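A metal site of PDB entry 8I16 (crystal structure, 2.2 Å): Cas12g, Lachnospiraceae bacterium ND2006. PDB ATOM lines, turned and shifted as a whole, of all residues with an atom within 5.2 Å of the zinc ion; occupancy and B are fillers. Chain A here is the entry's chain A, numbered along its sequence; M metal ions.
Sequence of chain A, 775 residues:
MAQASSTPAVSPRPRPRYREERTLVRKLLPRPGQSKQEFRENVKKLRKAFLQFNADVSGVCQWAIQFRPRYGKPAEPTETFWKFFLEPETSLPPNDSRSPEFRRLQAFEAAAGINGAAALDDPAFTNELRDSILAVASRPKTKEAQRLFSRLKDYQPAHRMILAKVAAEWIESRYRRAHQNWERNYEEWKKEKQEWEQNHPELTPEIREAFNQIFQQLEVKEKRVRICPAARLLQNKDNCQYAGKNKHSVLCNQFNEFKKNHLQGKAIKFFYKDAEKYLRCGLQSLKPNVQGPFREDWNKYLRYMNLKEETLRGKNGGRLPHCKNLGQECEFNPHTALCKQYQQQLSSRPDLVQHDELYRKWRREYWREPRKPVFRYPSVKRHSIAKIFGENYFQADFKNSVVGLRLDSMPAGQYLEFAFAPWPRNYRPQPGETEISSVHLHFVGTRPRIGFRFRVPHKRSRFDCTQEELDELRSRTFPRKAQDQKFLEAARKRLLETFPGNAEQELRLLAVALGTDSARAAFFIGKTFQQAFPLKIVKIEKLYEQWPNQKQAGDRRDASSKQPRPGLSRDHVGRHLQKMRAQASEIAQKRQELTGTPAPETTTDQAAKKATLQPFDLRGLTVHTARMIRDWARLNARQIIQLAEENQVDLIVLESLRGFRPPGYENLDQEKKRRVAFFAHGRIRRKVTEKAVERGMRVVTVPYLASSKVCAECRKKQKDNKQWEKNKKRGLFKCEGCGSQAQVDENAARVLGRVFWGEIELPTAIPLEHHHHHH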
ATOM      1  N   HIS A 248      13.897  28.643 -14.437  1.00  0.00           N
ATOM      2  CA  HIS A 248      14.565  27.567 -13.640  1.00  0.00           C
ATOM      3  C   HIS A 248      13.522  26.518 -13.249  1.00  0.00           C
ATOM      4  O   HIS A 248      12.345  26.840 -13.278  1.00  0.00           O
ATOM      5  CB  HIS A 248      15.193  28.094 -12.348  1.00  0.00           C
ATOM      6  CG  HIS A 248      16.376  28.983 -12.511  1.00  0.00           C
ATOM      7  ND1 HIS A 248      17.670  28.502 -12.406  1.00  0.00           N
ATOM      8  CD2 HIS A 248      16.471  30.322 -12.657  1.00  0.00           C
ATOM      9  CE1 HIS A 248      18.511  29.502 -12.533  1.00  0.00           C
ATOM     10  NE2 HIS A 248      17.808  30.640 -12.685  1.00  0.00           N
ATOM     11  N   SER A 249      13.962  25.335 -12.827  1.00  0.00           N
ATOM     12  CA  SER A 249      13.091  24.292 -12.214  1.00  0.00           C
ATOM     13  C   SER A 249      12.448  24.822 -10.920  1.00  0.00           C
ATOM     14  O   SER A 249      12.949  25.829 -10.327  1.00  0.00           O
ATOM     15  CB  SER A 249      13.882  22.988 -12.014  1.00  0.00           C
ATOM     16  OG  SER A 249      13.497  22.295 -10.841  1.00  0.00           O
ATOM     17  N   CYS A 252      14.853  24.719  -7.988  1.00  0.00           N
ATOM     18  CA  CYS A 252      15.808  25.867  -7.970  1.00  0.00           C
ATOM     19  C   CYS A 252      15.167  27.054  -7.258  1.00  0.00           C
ATOM     20  O   CYS A 252      15.911  27.808  -6.591  1.00  0.00           O
ATOM     21  CB  CYS A 252      16.276  26.257  -9.367  1.00  0.00           C
ATOM     22  SG  CYS A 252      16.576  24.838 -10.467  1.00  0.00           S
ATOM     23  N   HIS A 322      19.409  20.943  -8.597  1.00  0.00           N
ATOM     24  CA  HIS A 322      18.873  22.308  -8.710  1.00  0.00           C
ATOM     25  C   HIS A 322      20.051  23.259  -8.784  1.00  0.00           C
ATOM     26  O   HIS A 322      21.125  22.882  -8.321  1.00  0.00           O
ATOM     27  CB  HIS A 322      17.936  22.636  -7.537  1.00  0.00           C
ATOM     28  CG  HIS A 322      18.580  22.559  -6.193  1.00  0.00           C
ATOM     29  ND1 HIS A 322      19.426  23.554  -5.701  1.00  0.00           N
ATOM     30  CD2 HIS A 322      18.483  21.630  -5.215  1.00  0.00           C
ATOM     31  CE1 HIS A 322      19.831  23.229  -4.481  1.00  0.00           C
ATOM     32  NE2 HIS A 322      19.269  22.054  -4.158  1.00  0.00           N
ATOM     33  N   CYS A 323      19.819  24.432  -9.366  1.00  0.00           N
ATOM     34  CA  CYS A 323      20.792  25.525  -9.514  1.00  0.00           C
ATOM     35  C   CYS A 323      21.150  25.991  -8.083  1.00  0.00           C
ATOM     36  O   CYS A 323      20.433  25.612  -7.116  1.00  0.00           O
ATOM     37  CB  CYS A 323      20.204  26.567 -10.468  1.00  0.00           C
ATOM     38  SG  CYS A 323      20.030  25.960 -12.184  1.00  0.00           S
ATOM     39  N   ASN A 325      22.172  29.406  -7.631  1.00  0.00           N
ATOM     40  CA  ASN A 325      21.662  30.798  -7.798  1.00  0.00           C
ATOM     41  C   ASN A 325      20.408  30.765  -8.681  1.00  0.00           C
ATOM     42  O   ASN A 325      20.207  29.751  -9.388  1.00  0.00           O
ATOM     43  CB  ASN A 325      22.646  31.725  -8.517  1.00  0.00           C
ATOM     44  CG  ASN A 325      23.810  32.146  -7.648  1.00  0.00           C
ATOM     45  OD1 ASN A 325      23.651  32.959  -6.742  1.00  0.00           O
ATOM     46  ND2 ASN A 325      24.991  31.622  -7.935  1.00  0.00           N
ATOM     47  N   CYS A 330      19.539  27.740 -15.951  1.00  0.00           N
ATOM     48  CA  CYS A 330      19.340  26.462 -15.276  1.00  0.00           C
ATOM     49  C   CYS A 330      19.617  25.241 -16.153  1.00  0.00           C
ATOM     50  O   CYS A 330      19.348  25.250 -17.355  1.00  0.00           O
ATOM     51  CB  CYS A 330      17.924  26.373 -14.694  1.00  0.00           C
ATOM     52  SG  CYS A 330      17.471  24.740 -14.084  1.00  0.00           S
ATOM     53  N   GLU A 331      20.169  24.198 -15.537  1.00  0.00           N
ATOM     54  CA  GLU A 331      20.491  22.927 -16.227  1.00  0.00           C
ATOM     55  C   GLU A 331      19.582  21.834 -15.662  1.00  0.00           C
ATOM     56  O   GLU A 331      19.806  20.648 -15.994  1.00  0.00           O
ATOM     57  CB  GLU A 331      21.985  22.603 -16.138  1.00  0.00           C
ATOM     58  CG  GLU A 331      22.661  22.933 -14.806  1.00  0.00           C
ATOM     59  CD  GLU A 331      23.499  24.204 -14.762  1.00  0.00           C
ATOM     60  OE1 GLU A 331      24.566  24.191 -14.084  1.00  0.00           O
ATOM     61  OE2 GLU A 331      23.101  25.215 -15.390  1.00  0.00           O
ATOM     62  N   PHE A 332      18.538  22.204 -14.897  1.00  0.00           N
ATOM     63  CA  PHE A 332      17.622  21.213 -14.263  1.00  0.00           C
ATOM     64  C   PHE A 332      16.206  21.444 -14.769  1.00  0.00           C
ATOM     65  O   PHE A 332      15.259  20.833 -14.223  1.00  0.00           O
ATOM     66  CB  PHE A 332      17.765  21.259 -12.737  1.00  0.00           C
ATOM     67  CG  PHE A 332      19.196  21.085 -12.289  1.00  0.00           C
ATOM     68  CD1 PHE A 332      19.766  19.818 -12.242  1.00  0.00           C
ATOM     69  CD2 PHE A 332      19.999  22.189 -12.034  1.00  0.00           C
ATOM     70  CE1 PHE A 332      21.102  19.671 -11.892  1.00  0.00           C
ATOM     71  CE2 PHE A 332      21.331  22.027 -11.689  1.00  0.00           C
ATOM     72  CZ  PHE A 332      21.884  20.769 -11.613  1.00  0.00           C
HETATM   73 ZN    ZN M   1      17.801  26.378 -11.989  1.00  0.00          ZN
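Within 4 Å of the zinc ion: His 248, Cys 252, Cys 323 and Cys 330.
The nearest printed residue that does not touch the zinc ion is Ser 249 (4.1 Å).
The zinc ion is bound by ND1 of His 248 (2.2 Å), SG of Cys 323 (2.3 Å), SG of Cys 252 (2.5 Å) and SG of Cys 330 (2.7 Å).
N of Glu 331 lies close to SG of Cys 323, 3.8 Å away.
The side-chain sulfur of Cys 252 lies close to the backbone NH of Ser 249, 3.6 Å away.
SG of Cys 330 sits close to N of Ser 249, 3.8 Å away.
N of Phe 332 lies close to SG of Cys 330 (2.9 Å).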
